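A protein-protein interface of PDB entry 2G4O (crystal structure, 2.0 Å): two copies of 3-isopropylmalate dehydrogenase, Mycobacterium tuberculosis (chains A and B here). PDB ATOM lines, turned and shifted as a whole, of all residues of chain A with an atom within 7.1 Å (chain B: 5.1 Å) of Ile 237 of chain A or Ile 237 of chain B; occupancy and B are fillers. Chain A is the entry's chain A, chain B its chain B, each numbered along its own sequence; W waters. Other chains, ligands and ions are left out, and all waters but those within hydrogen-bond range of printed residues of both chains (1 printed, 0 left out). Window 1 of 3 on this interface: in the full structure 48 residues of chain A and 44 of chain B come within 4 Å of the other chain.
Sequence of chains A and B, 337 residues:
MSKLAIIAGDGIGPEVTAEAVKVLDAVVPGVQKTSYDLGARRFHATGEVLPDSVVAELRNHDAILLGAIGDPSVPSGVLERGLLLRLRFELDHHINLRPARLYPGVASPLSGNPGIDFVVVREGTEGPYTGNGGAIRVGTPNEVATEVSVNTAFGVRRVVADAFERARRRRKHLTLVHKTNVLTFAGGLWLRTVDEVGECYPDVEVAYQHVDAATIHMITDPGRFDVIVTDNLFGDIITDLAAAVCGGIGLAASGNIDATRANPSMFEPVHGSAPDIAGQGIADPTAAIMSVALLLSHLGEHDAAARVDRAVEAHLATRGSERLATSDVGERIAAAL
Printed residues of chain B within 4 Å of Lys 179 of chain A: Asp 236. Of the printed residues of chain B, Asp 212 of chain A touches Asp 236 and Asp 240. Printed residues of chain B within 4 Å of Asp 236 of chain A: Asp 212 (3.8 Å). Of chain B, only Val 211, Thr 215 and Ile 237 come within 4 Å of Ile 237 of chain A. Phe 234 of chain B touches none of the printed residues of chain A. Of the printed residues of chain A, Asp 236 of chain B touches Lys 179 (3.2 Å) and Asp 212 (3.5 Å). Of the printed residues of chain A, Ile 237 of chain B touches Val 211 (3.9 Å), Thr 215 (3.9 Å) and Ile 237 (3.9 Å). The nearest residue of chain B that does not touch Ile 237 of chain A is Asp 212 of chain B (4.2 Å). The nearest residue of chain A that does not touch Ile 237 of chain B is Asp 212 of chain A (4.1 Å). The nearest printed residue of chain B that does not touch Leu 241 of chain A is Leu 241 of chain B (4.4 Å).
The side-chain hydroxyl (OH) of Tyr 129 of chain A lies close to the side-chain carboxylate (OD2) of Asp 236 of chain A (3.4 Å). NZ of Lys 179 of chain A is in salt-bridge range of OD1 of Asp 212 of chain A (3.2 Å). The side-chain hydroxyl (OG1) of Thr 215 of chain A sits at hydrogen-bond distance from the backbone carbonyl oxygen (O) of Val 211 of chain A, at 3.1 Å. The backbone carbonyl oxygen (O) of Asp 236 of chain A lies within hydrogen-bond range of the side-chain hydroxyl (OG1) of Thr 239 of chain A, at 3.3 Å. The backbone carbonyl oxygen (O) of Asp 212 of chain B is in hydrogen-bond range of the side-chain hydroxyl (OG1) of Thr 215 of chain B (2.7 Å). The side-chain hydroxyl of Thr 239 of chain B is in hydrogen-bond range of the backbone carbonyl oxygen of Asp 236 of chain B (3.3 Å).
Val 211 of chain A touches Ile 237 of chain B, and with the chains exchanged Ile 237 of chain A touches Val 211 of chain B. Asp 212 of chain A touches Asp 236 of chain B, and with the chains exchanged Asp 236 of chain A touches Asp 212 of chain B. Thr 215 of chain A touches Ile 237 of chain B, and with the chains exchanged Ile 237 of chain A touches Thr 215 of chain B. Ile 237 of chain B touches its own counterpart, Ile 237 of chain A. Positions printed for both chains: 211, 212, 215, 233, 234, 235, 236, 237, 238, 239, 240 and 241.
The side-chain carboxylate of Asp 236 of chain B is in salt-bridge range of the side-chain amino group of Lys 179 of chain A (3.2 Å). OD2 of Asp 236 of chain B lies close to OD2 of Asp 212 of chain A (3.5 Å). The side-chain carboxylate of Asp 212 of chain A sits close to the side-chain carboxylate of Asp 240 of chain B (2.8 Å). The side-chain carboxylate of Asp 240 of chain A lies close to the side-chain carboxylate of Asp 212 of chain B (3.1 Å).
Water W1 lies within hydrogen-bond range of the side-chain carboxylate of Asp 236 of chain B, the backbone NH of Asp 212 of chain A and the side-chain amino group of Lys 179 of chain A.
Among the printed residues, pairs that only touch across the chains: Val 211 of chain A with Ile 237 of chain B, Thr 215 of chain A with Ile 237 of chain B, Thr 215 of chain A with Leu 241 of chain B, Ile 216 of chain A with Asp 240 of chain B, Asp 236 of chain A with Asp 212 of chain B, Ile 237 of chain A with Val 211 of chain B, Ile 237 of chain A with Thr 215 of chain B, Ile 237 of chain A with Ile 237 of chain B and Leu 241 of chain A with Thr 215 of chain B.
Of the 22 printed residues of chain A, 9 touch a printed residue of chain B. Printed residues of chain A that touch a printed residue of chain B: Lys 179, Val 211, Asp 212, Thr 215, Ile 216, Asp 236, Ile 237, Asp 240 and Leu 241. Hydrophobic or aromatic side chains of chain A within 4 Å of the printed part of chain B: Val 211, Ile 216, Ile 237 and Leu 241. Along chain A the printed residues that touch a printed residue of chain B span positions 179 to 241. Among the printed residues, Asp or Glu carboxylates within 4 Å of a Lys or Arg side-chain nitrogen of the other chain: Lys 179 of chain A with Asp 236 of chain B.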
ATOM      1  N   ARG A 122     -28.280  13.785 -29.881  1.00  0.00           N
ATOM      2  CA  ARG A 122     -28.710  12.600 -29.118  1.00  0.00           C
ATOM      3  C   ARG A 122     -29.672  11.793 -29.986  1.00  0.00           C
ATOM      4  O   ARG A 122     -30.665  12.352 -30.525  1.00  0.00           O
ATOM      5  CB  ARG A 122     -29.380  13.081 -27.861  1.00  0.00           C
ATOM      6  CG  ARG A 122     -30.285  12.148 -27.124  1.00  0.00           C
ATOM      7  CD  ARG A 122     -30.975  12.813 -25.985  1.00  0.00           C
ATOM      8  NE  ARG A 122     -31.799  11.850 -25.198  1.00  0.00           N
ATOM      9  CZ  ARG A 122     -32.836  12.195 -24.448  1.00  0.00           C
ATOM     10  NH1 ARG A 122     -33.535  11.259 -23.827  1.00  0.00           N
ATOM     11  NH2 ARG A 122     -33.242  13.443 -24.406  1.00  0.00           N
ATOM     12  N   TYR A 129     -34.641   3.811 -23.578  1.00  0.00           N
ATOM     13  CA  TYR A 129     -35.679   4.701 -23.184  1.00  0.00           C
ATOM     14  C   TYR A 129     -36.989   4.354 -23.918  1.00  0.00           C
ATOM     15  O   TYR A 129     -37.953   5.149 -23.976  1.00  0.00           O
ATOM     16  CB  TYR A 129     -35.182   6.159 -23.390  1.00  0.00           C
ATOM     17  CG  TYR A 129     -34.381   6.708 -22.197  1.00  0.00           C
ATOM     18  CD1 TYR A 129     -34.013   5.880 -21.105  1.00  0.00           C
ATOM     19  CD2 TYR A 129     -34.010   8.044 -22.141  1.00  0.00           C
ATOM     20  CE1 TYR A 129     -33.290   6.377 -20.009  1.00  0.00           C
ATOM     21  CE2 TYR A 129     -33.285   8.548 -21.064  1.00  0.00           C
ATOM     22  CZ  TYR A 129     -32.927   7.722 -19.986  1.00  0.00           C
ATOM     23  OH  TYR A 129     -32.212   8.206 -18.869  1.00  0.00           O
ATOM     24  N   LYS A 179     -20.055   4.055 -23.850  1.00  0.00           N
ATOM     25  CA  LYS A 179     -19.408   3.312 -22.762  1.00  0.00           C
ATOM     26  C   LYS A 179     -19.104   1.909 -23.312  1.00  0.00           C
ATOM     27  O   LYS A 179     -19.646   0.859 -22.867  1.00  0.00           O
ATOM     28  CB  LYS A 179     -20.266   3.233 -21.511  1.00  0.00           C
ATOM     29  CG  LYS A 179     -19.485   2.719 -20.315  1.00  0.00           C
ATOM     30  CD  LYS A 179     -18.585   3.789 -19.665  1.00  0.00           C
ATOM     31  CE  LYS A 179     -17.319   3.175 -19.062  1.00  0.00           C
ATOM     32  NZ  LYS A 179     -16.870   3.876 -17.854  1.00  0.00           N
ATOM     33  N   VAL A 211     -18.642   8.104 -21.311  1.00  0.00           N
ATOM     34  CA  VAL A 211     -19.572   9.049 -20.738  1.00  0.00           C
ATOM     35  C   VAL A 211     -19.116   9.622 -19.377  1.00  0.00           C
ATOM     36  O   VAL A 211     -19.306  10.805 -19.130  1.00  0.00           O
ATOM     37  CB  VAL A 211     -21.010   8.457 -20.654  1.00  0.00           C
ATOM     38  CG1 VAL A 211     -21.081   7.209 -19.840  1.00  0.00           C
ATOM     39  CG2 VAL A 211     -21.945   9.474 -20.103  1.00  0.00           C
ATOM     40  N   ASP A 212     -18.524   8.806 -18.502  1.00  0.00           N
ATOM     41  CA  ASP A 212     -17.994   9.335 -17.257  1.00  0.00           C
ATOM     42  C   ASP A 212     -16.838  10.308 -17.492  1.00  0.00           C
ATOM     43  O   ASP A 212     -16.821  11.364 -16.890  1.00  0.00           O
ATOM     44  CB  ASP A 212     -17.666   8.251 -16.233  1.00  0.00           C
ATOM     45  CG  ASP A 212     -16.679   7.214 -16.719  1.00  0.00           C
ATOM     46  OD1 ASP A 212     -16.483   7.071 -17.944  1.00  0.00           O
ATOM     47  OD2 ASP A 212     -16.136   6.481 -15.846  1.00  0.00           O
ATOM     48  N   ALA A 213     -15.903   9.997 -18.399  1.00  0.00           N
ATOM     49  CA  ALA A 213     -14.843  10.946 -18.747  1.00  0.00           C
ATOM     50  C   ALA A 213     -15.375  12.190 -19.467  1.00  0.00           C
ATOM     51  O   ALA A 213     -14.874  13.312 -19.261  1.00  0.00           O
ATOM     52  CB  ALA A 213     -13.785  10.276 -19.618  1.00  0.00           C
ATOM     53  N   THR A 215     -18.214  13.582 -18.976  1.00  0.00           N
ATOM     54  CA  THR A 215     -18.891  14.327 -17.914  1.00  0.00           C
ATOM     55  C   THR A 215     -17.825  15.185 -17.223  1.00  0.00           C
ATOM     56  O   THR A 215     -17.997  16.369 -17.044  1.00  0.00           O
ATOM     57  CB  THR A 215     -19.646  13.278 -16.986  1.00  0.00           C
ATOM     58  OG1 THR A 215     -20.939  12.879 -17.580  1.00  0.00           O
ATOM     59  CG2 THR A 215     -19.864  13.762 -15.640  1.00  0.00           C
ATOM     60  N   ILE A 216     -16.678  14.585 -16.908  1.00  0.00           N
ATOM     61  CA  ILE A 216     -15.576  15.320 -16.330  1.00  0.00           C
ATOM     62  C   ILE A 216     -15.089  16.451 -17.224  1.00  0.00           C
ATOM     63  O   ILE A 216     -14.942  17.592 -16.776  1.00  0.00           O
ATOM     64  CB  ILE A 216     -14.388  14.393 -16.015  1.00  0.00           C
ATOM     65  CG1 ILE A 216     -14.817  13.341 -14.975  1.00  0.00           C
ATOM     66  CG2 ILE A 216     -13.142  15.246 -15.538  1.00  0.00           C
ATOM     67  CD1 ILE A 216     -13.706  12.401 -14.523  1.00  0.00           C
ATOM     68  N   MET A 218     -16.697  18.066 -19.582  1.00  0.00           N
ATOM     69  CA  MET A 218     -17.713  19.151 -19.687  1.00  0.00           C
ATOM     70  C   MET A 218     -17.582  20.201 -18.530  1.00  0.00           C
ATOM     71  O   MET A 218     -18.050  21.358 -18.639  1.00  0.00           O
ATOM     72  CB  MET A 218     -19.123  18.531 -19.740  1.00  0.00           C
ATOM     73  CG  MET A 218     -20.140  19.263 -20.556  1.00  0.00           C
ATOM     74  SD  MET A 218     -21.540  18.187 -21.036  1.00  0.00           S
ATOM     75  CE  MET A 218     -20.910  17.180 -22.370  1.00  0.00           C
ATOM     76  N   ASP A 231     -26.072   8.322 -27.646  1.00  0.00           N
ATOM     77  CA  ASP A 231     -27.318   7.597 -27.587  1.00  0.00           C
ATOM     78  C   ASP A 231     -28.381   8.294 -26.704  1.00  0.00           C
ATOM     79  O   ASP A 231     -28.152   9.386 -26.124  1.00  0.00           O
ATOM     80  CB  ASP A 231     -27.094   6.118 -27.203  1.00  0.00           C
ATOM     81  CG  ASP A 231     -27.036   5.861 -25.687  1.00  0.00           C
ATOM     82  OD1 ASP A 231     -26.761   6.781 -24.909  1.00  0.00           O
ATOM     83  OD2 ASP A 231     -27.282   4.694 -25.249  1.00  0.00           O
ATOM     84  N   ASN A 232     -29.530   7.640 -26.593  1.00  0.00           N
ATOM     85  CA  ASN A 232     -30.734   8.228 -25.962  1.00  0.00           C
ATOM     86  C   ASN A 232     -30.489   8.425 -24.467  1.00  0.00           C
ATOM     87  O   ASN A 232     -30.716   9.506 -23.924  1.00  0.00           O
ATOM     88  CB  ASN A 232     -31.941   7.300 -26.236  1.00  0.00           C
ATOM     89  CG  ASN A 232     -33.305   7.997 -26.208  1.00  0.00           C
ATOM     90  OD1 ASN A 232     -33.481   9.126 -25.702  1.00  0.00           O
ATOM     91  ND2 ASN A 232     -34.310   7.293 -26.795  1.00  0.00           N
ATOM     92  N   LEU A 233     -29.973   7.399 -23.783  1.00  0.00           N
ATOM     93  CA  LEU A 233     -29.789   7.463 -22.352  1.00  0.00           C
ATOM     94  C   LEU A 233     -28.605   8.369 -21.931  1.00  0.00           C
ATOM     95  O   LEU A 233     -28.750   9.244 -21.068  1.00  0.00           O
ATOM     96  CB  LEU A 233     -29.560   6.062 -21.814  1.00  0.00           C
ATOM     97  CG  LEU A 233     -29.307   5.896 -20.268  1.00  0.00           C
ATOM     98  CD1 LEU A 233     -29.495   4.478 -19.787  1.00  0.00           C
ATOM     99  CD2 LEU A 233     -27.943   6.336 -19.816  1.00  0.00           C
ATOM    100  N   PHE A 234     -27.422   8.152 -22.532  1.00  0.00           N
ATOM    101  CA  PHE A 234     -26.293   8.953 -22.174  1.00  0.00           C
ATOM    102  C   PHE A 234     -26.588  10.405 -22.623  1.00  0.00           C
ATOM    103  O   PHE A 234     -26.256  11.369 -21.926  1.00  0.00           O
ATOM    104  CB  PHE A 234     -24.969   8.443 -22.819  1.00  0.00           C
ATOM    105  CG  PHE A 234     -24.532   7.104 -22.344  1.00  0.00           C
ATOM    106  CD1 PHE A 234     -24.634   6.708 -21.013  1.00  0.00           C
ATOM    107  CD2 PHE A 234     -23.958   6.225 -23.230  1.00  0.00           C
ATOM    108  CE1 PHE A 234     -24.247   5.443 -20.612  1.00  0.00           C
ATOM    109  CE2 PHE A 234     -23.569   4.988 -22.830  1.00  0.00           C
ATOM    110  CZ  PHE A 234     -23.710   4.589 -21.519  1.00  0.00           C
ATOM    111  N   GLY A 235     -27.219  10.569 -23.753  1.00  0.00           N
ATOM    112  CA  GLY A 235     -27.560  11.918 -24.230  1.00  0.00           C
ATOM    113  C   GLY A 235     -28.483  12.663 -23.303  1.00  0.00           C
ATOM    114  O   GLY A 235     -28.378  13.859 -23.133  1.00  0.00           O
ATOM    115  N   ASP A 236     -29.368  11.940 -22.655  1.00  0.00           N
ATOM    116  CA  ASP A 236     -30.309  12.552 -21.731  1.00  0.00           C
ATOM    117  C   ASP A 236     -29.559  13.281 -20.649  1.00  0.00           C
ATOM    118  O   ASP A 236     -29.935  14.395 -20.270  1.00  0.00           O
ATOM    119  CB  ASP A 236     -31.186  11.486 -21.046  1.00  0.00           C
ATOM    120  CG  ASP A 236     -32.553  12.034 -20.553  1.00  0.00           C
ATOM    121  OD1 ASP A 236     -32.992  13.163 -20.928  1.00  0.00           O
ATOM    122  OD2 ASP A 236     -33.174  11.326 -19.731  1.00  0.00           O
ATOM    123  N   ILE A 237     -28.534  12.621 -20.119  1.00  0.00           N
ATOM    124  CA  ILE A 237     -27.735  13.138 -19.020  1.00  0.00           C
ATOM    125  C   ILE A 237     -26.821  14.267 -19.493  1.00  0.00           C
ATOM    126  O   ILE A 237     -26.809  15.374 -18.874  1.00  0.00           O
ATOM    127  CB  ILE A 237     -26.915  12.015 -18.380  1.00  0.00           C
ATOM    128  CG1 ILE A 237     -27.859  10.993 -17.761  1.00  0.00           C
ATOM    129  CG2 ILE A 237     -25.988  12.507 -17.290  1.00  0.00           C
ATOM    130  CD1 ILE A 237     -27.129   9.764 -17.191  1.00  0.00           C
ATOM    131  N   ILE A 238     -26.075  14.023 -20.573  1.00  0.00           N
ATOM    132  CA  ILE A 238     -25.097  15.037 -20.986  1.00  0.00           C
ATOM    133  C   ILE A 238     -25.694  16.325 -21.603  1.00  0.00           C
ATOM    134  O   ILE A 238     -25.104  17.361 -21.416  1.00  0.00           O
ATOM    135  CB  ILE A 238     -23.895  14.503 -21.796  1.00  0.00           C
ATOM    136  CG1 ILE A 238     -24.229  14.301 -23.203  1.00  0.00           C
ATOM    137  CG2 ILE A 238     -23.290  13.180 -21.245  1.00  0.00           C
ATOM    138  CD1 ILE A 238     -23.573  15.342 -24.000  1.00  0.00           C
ATOM    139  N   THR A 239     -26.885  16.263 -22.208  1.00  0.00           N
ATOM    140  CA  THR A 239     -27.576  17.459 -22.733  1.00  0.00           C
ATOM    141  C   THR A 239     -28.004  18.365 -21.582  1.00  0.00           C
ATOM    142  O   THR A 239     -27.834  19.560 -21.701  1.00  0.00           O
ATOM    143  CB  THR A 239     -28.735  17.130 -23.588  1.00  0.00           C
ATOM    144  OG1 THR A 239     -29.715  16.331 -22.879  1.00  0.00           O
ATOM    145  CG2 THR A 239     -28.228  16.371 -24.858  1.00  0.00           C
ATOM    146  N   ASP A 240     -28.457  17.771 -20.456  1.00  0.00           N
ATOM    147  CA  ASP A 240     -28.758  18.511 -19.231  1.00  0.00           C
ATOM    148  C   ASP A 240     -27.547  19.085 -18.492  1.00  0.00           C
ATOM    149  O   ASP A 240     -27.604  20.209 -18.006  1.00  0.00           O
ATOM    150  CB  ASP A 240     -29.607  17.691 -18.280  1.00  0.00           C
ATOM    151  CG  ASP A 240     -31.106  17.746 -18.648  1.00  0.00           C
ATOM    152  OD1 ASP A 240     -31.501  18.158 -19.785  1.00  0.00           O
ATOM    153  OD2 ASP A 240     -31.883  17.337 -17.800  1.00  0.00           O
ATOM    154  N   LEU A 241     -26.466  18.324 -18.436  1.00  0.00           N
ATOM    155  CA  LEU A 241     -25.206  18.834 -17.987  1.00  0.00           C
ATOM    156  C   LEU A 241     -24.676  19.943 -18.863  1.00  0.00           C
ATOM    157  O   LEU A 241     -24.210  20.967 -18.346  1.00  0.00           O
ATOM    158  CB  LEU A 241     -24.181  17.692 -17.832  1.00  0.00           C
ATOM    159  CG  LEU A 241     -22.822  18.063 -17.209  1.00  0.00           C
ATOM    160  CD1 LEU A 241     -23.012  18.447 -15.751  1.00  0.00           C
ATOM    161  CD2 LEU A 241     -21.877  16.859 -17.362  1.00  0.00           C
ATOM    162  N   ALA A 242     -24.856  19.850 -20.184  1.00  0.00           N
ATOM    163  CA  ALA A 242     -24.394  20.906 -21.045  1.00  0.00           C
ATOM    164  C   ALA A 242     -25.111  22.173 -20.670  1.00  0.00           C
ATOM    165  O   ALA A 242     -24.489  23.240 -20.566  1.00  0.00           O
ATOM    166  CB  ALA A 242     -24.602  20.562 -22.485  1.00  0.00           C
ATOM    167  N   ALA A 243     -26.416  22.043 -20.477  1.00  0.00           N
ATOM    168  CA  ALA A 243     -27.314  23.176 -20.218  1.00  0.00           C
ATOM    169  C   ALA A 243     -26.862  23.853 -18.965  1.00  0.00           C
ATOM    170  O   ALA A 243     -26.715  25.100 -18.951  1.00  0.00           O
ATOM    171  CB  ALA A 243     -28.784  22.725 -20.104  1.00  0.00           C
ATOM    172  N   VAL B 211     -31.342  11.103 -12.674  1.00  0.00           N
ATOM    173  CA  VAL B 211     -29.916  11.254 -12.848  1.00  0.00           C
ATOM    174  C   VAL B 211     -29.490  12.525 -13.614  1.00  0.00           C
ATOM    175  O   VAL B 211     -28.427  13.104 -13.335  1.00  0.00           O
ATOM    176  CB  VAL B 211     -29.354   9.954 -13.480  1.00  0.00           C
ATOM    177  CG1 VAL B 211     -30.141   9.634 -14.775  1.00  0.00           C
ATOM    178  CG2 VAL B 211     -27.875  10.067 -13.729  1.00  0.00           C
ATOM    179  N   ASP B 212     -30.319  12.971 -14.543  1.00  0.00           N
ATOM    180  CA  ASP B 212     -30.019  14.176 -15.287  1.00  0.00           C
ATOM    181  C   ASP B 212     -30.018  15.421 -14.354  1.00  0.00           C
ATOM    182  O   ASP B 212     -29.074  16.209 -14.392  1.00  0.00           O
ATOM    183  CB  ASP B 212     -30.932  14.361 -16.559  1.00  0.00           C
ATOM    184  CG  ASP B 212     -32.397  14.178 -16.317  1.00  0.00           C
ATOM    185  OD1 ASP B 212     -32.786  13.582 -15.295  1.00  0.00           O
ATOM    186  OD2 ASP B 212     -33.205  14.620 -17.208  1.00  0.00           O
ATOM    187  N   THR B 215     -27.057  15.435 -11.899  1.00  0.00           N
ATOM    188  CA  THR B 215     -25.821  15.900 -12.529  1.00  0.00           C
ATOM    189  C   THR B 215     -25.769  17.443 -12.568  1.00  0.00           C
ATOM    190  O   THR B 215     -24.707  18.009 -12.325  1.00  0.00           O
ATOM    191  CB  THR B 215     -25.534  15.337 -13.964  1.00  0.00           C
ATOM    192  OG1 THR B 215     -26.441  15.917 -14.915  1.00  0.00           O
ATOM    193  CG2 THR B 215     -25.599  13.818 -13.956  1.00  0.00           C
ATOM    194  N   LEU B 233     -24.662   1.526 -13.295  1.00  0.00           N
ATOM    195  CA  LEU B 233     -24.528   2.423 -14.454  1.00  0.00           C
ATOM    196  C   LEU B 233     -24.586   3.893 -14.087  1.00  0.00           C
ATOM    197  O   LEU B 233     -23.639   4.610 -14.382  1.00  0.00           O
ATOM    198  CB  LEU B 233     -25.565   2.101 -15.553  1.00  0.00           C
ATOM    199  CG  LEU B 233     -25.439   2.905 -16.866  1.00  0.00           C
ATOM    200  CD1 LEU B 233     -26.335   2.423 -18.022  1.00  0.00           C
ATOM    201  CD2 LEU B 233     -25.742   4.348 -16.650  1.00  0.00           C
ATOM    202  N   PHE B 234     -25.663   4.383 -13.488  1.00  0.00           N
ATOM    203  CA  PHE B 234     -25.666   5.775 -13.052  1.00  0.00           C
ATOM    204  C   PHE B 234     -24.543   6.144 -12.034  1.00  0.00           C
ATOM    205  O   PHE B 234     -23.980   7.236 -12.116  1.00  0.00           O
ATOM    206  CB  PHE B 234     -27.052   6.228 -12.526  1.00  0.00           C
ATOM    207  CG  PHE B 234     -28.212   6.028 -13.515  1.00  0.00           C
ATOM    208  CD1 PHE B 234     -28.065   6.336 -14.862  1.00  0.00           C
ATOM    209  CD2 PHE B 234     -29.454   5.590 -13.083  1.00  0.00           C
ATOM    210  CE1 PHE B 234     -29.156   6.181 -15.764  1.00  0.00           C
ATOM    211  CE2 PHE B 234     -30.558   5.453 -13.980  1.00  0.00           C
ATOM    212  CZ  PHE B 234     -30.415   5.729 -15.275  1.00  0.00           C
ATOM    213  N   GLY B 235     -24.178   5.235 -11.131  1.00  0.00           N
ATOM    214  CA  GLY B 235     -23.089   5.490 -10.163  1.00  0.00           C
ATOM    215  C   GLY B 235     -21.719   5.657 -10.826  1.00  0.00           C
ATOM    216  O   GLY B 235     -20.876   6.435 -10.402  1.00  0.00           O
ATOM    217  N   ASP B 236     -21.512   4.938 -11.902  1.00  0.00           N
ATOM    218  CA  ASP B 236     -20.269   5.013 -12.620  1.00  0.00           C
ATOM    219  C   ASP B 236     -20.096   6.415 -13.163  1.00  0.00           C
ATOM    220  O   ASP B 236     -18.979   6.963 -13.188  1.00  0.00           O
ATOM    221  CB  ASP B 236     -20.272   3.966 -13.734  1.00  0.00           C
ATOM    222  CG  ASP B 236     -18.981   3.950 -14.511  1.00  0.00           C
ATOM    223  OD1 ASP B 236     -17.958   3.463 -13.967  1.00  0.00           O
ATOM    224  OD2 ASP B 236     -19.009   4.513 -15.624  1.00  0.00           O
ATOM    225  N   ILE B 237     -21.204   7.040 -13.543  1.00  0.00           N
ATOM    226  CA  ILE B 237     -21.134   8.374 -14.079  1.00  0.00           C
ATOM    227  C   ILE B 237     -21.081   9.441 -12.968  1.00  0.00           C
ATOM    228  O   ILE B 237     -20.330  10.464 -13.027  1.00  0.00           O
ATOM    229  CB  ILE B 237     -22.398   8.655 -14.979  1.00  0.00           C
ATOM    230  CG1 ILE B 237     -22.389   7.794 -16.222  1.00  0.00           C
ATOM    231  CG2 ILE B 237     -22.421  10.056 -15.392  1.00  0.00           C
ATOM    232  CD1 ILE B 237     -23.697   7.898 -17.030  1.00  0.00           C
ATOM    233  N   ILE B 238     -21.911   9.268 -11.966  1.00  0.00           N
ATOM    234  CA  ILE B 238     -21.923  10.317 -11.010  1.00  0.00           C
ATOM    235  C   ILE B 238     -20.650  10.259 -10.118  1.00  0.00           C
ATOM    236  O   ILE B 238     -20.247  11.309  -9.631  1.00  0.00           O
ATOM    237  CB  ILE B 238     -23.202  10.475 -10.195  1.00  0.00           C
ATOM    238  CG1 ILE B 238     -23.474   9.288  -9.311  1.00  0.00           C
ATOM    239  CG2 ILE B 238     -24.443  10.819 -11.085  1.00  0.00           C
ATOM    240  CD1 ILE B 238     -24.651   9.568  -8.442  1.00  0.00           C
ATOM    241  N   THR B 239     -19.986   9.098 -10.005  1.00  0.00           N
ATOM    242  CA  THR B 239     -18.799   9.010  -9.130  1.00  0.00           C
ATOM    243  C   THR B 239     -17.645   9.804  -9.735  1.00  0.00           C
ATOM    244  O   THR B 239     -16.887  10.513  -9.034  1.00  0.00           O
ATOM    245  CB  THR B 239     -18.340   7.572  -8.798  1.00  0.00           C
ATOM    246  OG1 THR B 239     -18.080   6.807  -9.988  1.00  0.00           O
ATOM    247  CG2 THR B 239     -19.307   6.887  -7.944  1.00  0.00           C
ATOM    248  N   ASP B 240     -17.526   9.725 -11.053  1.00  0.00           N
ATOM    249  CA  ASP B 240     -16.479  10.417 -11.718  1.00  0.00           C
ATOM    250  C   ASP B 240     -16.698  11.917 -11.709  1.00  0.00           C
ATOM    251  O   ASP B 240     -15.711  12.686 -11.561  1.00  0.00           O
ATOM    252  CB  ASP B 240     -16.293   9.874 -13.134  1.00  0.00           C
ATOM    253  CG  ASP B 240     -15.414   8.666 -13.151  1.00  0.00           C
ATOM    254  OD1 ASP B 240     -15.322   8.032 -12.060  1.00  0.00           O
ATOM    255  OD2 ASP B 240     -14.802   8.383 -14.216  1.00  0.00           O
ATOM    256  N   LEU B 241     -17.962  12.335 -11.809  1.00  0.00           N
ATOM    257  CA  LEU B 241     -18.303  13.746 -11.786  1.00  0.00           C
ATOM    258  C   LEU B 241     -18.039  14.351 -10.424  1.00  0.00           C
ATOM    259  O   LEU B 241     -17.534  15.465 -10.348  1.00  0.00           O
ATOM    260  CB  LEU B 241     -19.771  13.997 -12.125  1.00  0.00           C
ATOM    261  CG  LEU B 241     -20.197  15.454 -12.221  1.00  0.00           C
ATOM    262  CD1 LEU B 241     -19.212  16.295 -13.047  1.00  0.00           C
ATOM    263  CD2 LEU B 241     -21.592  15.533 -12.831  1.00  0.00           C
HETATM  264  O   HOH W   1     -19.506   5.832 -17.594  1.00  0.00           O
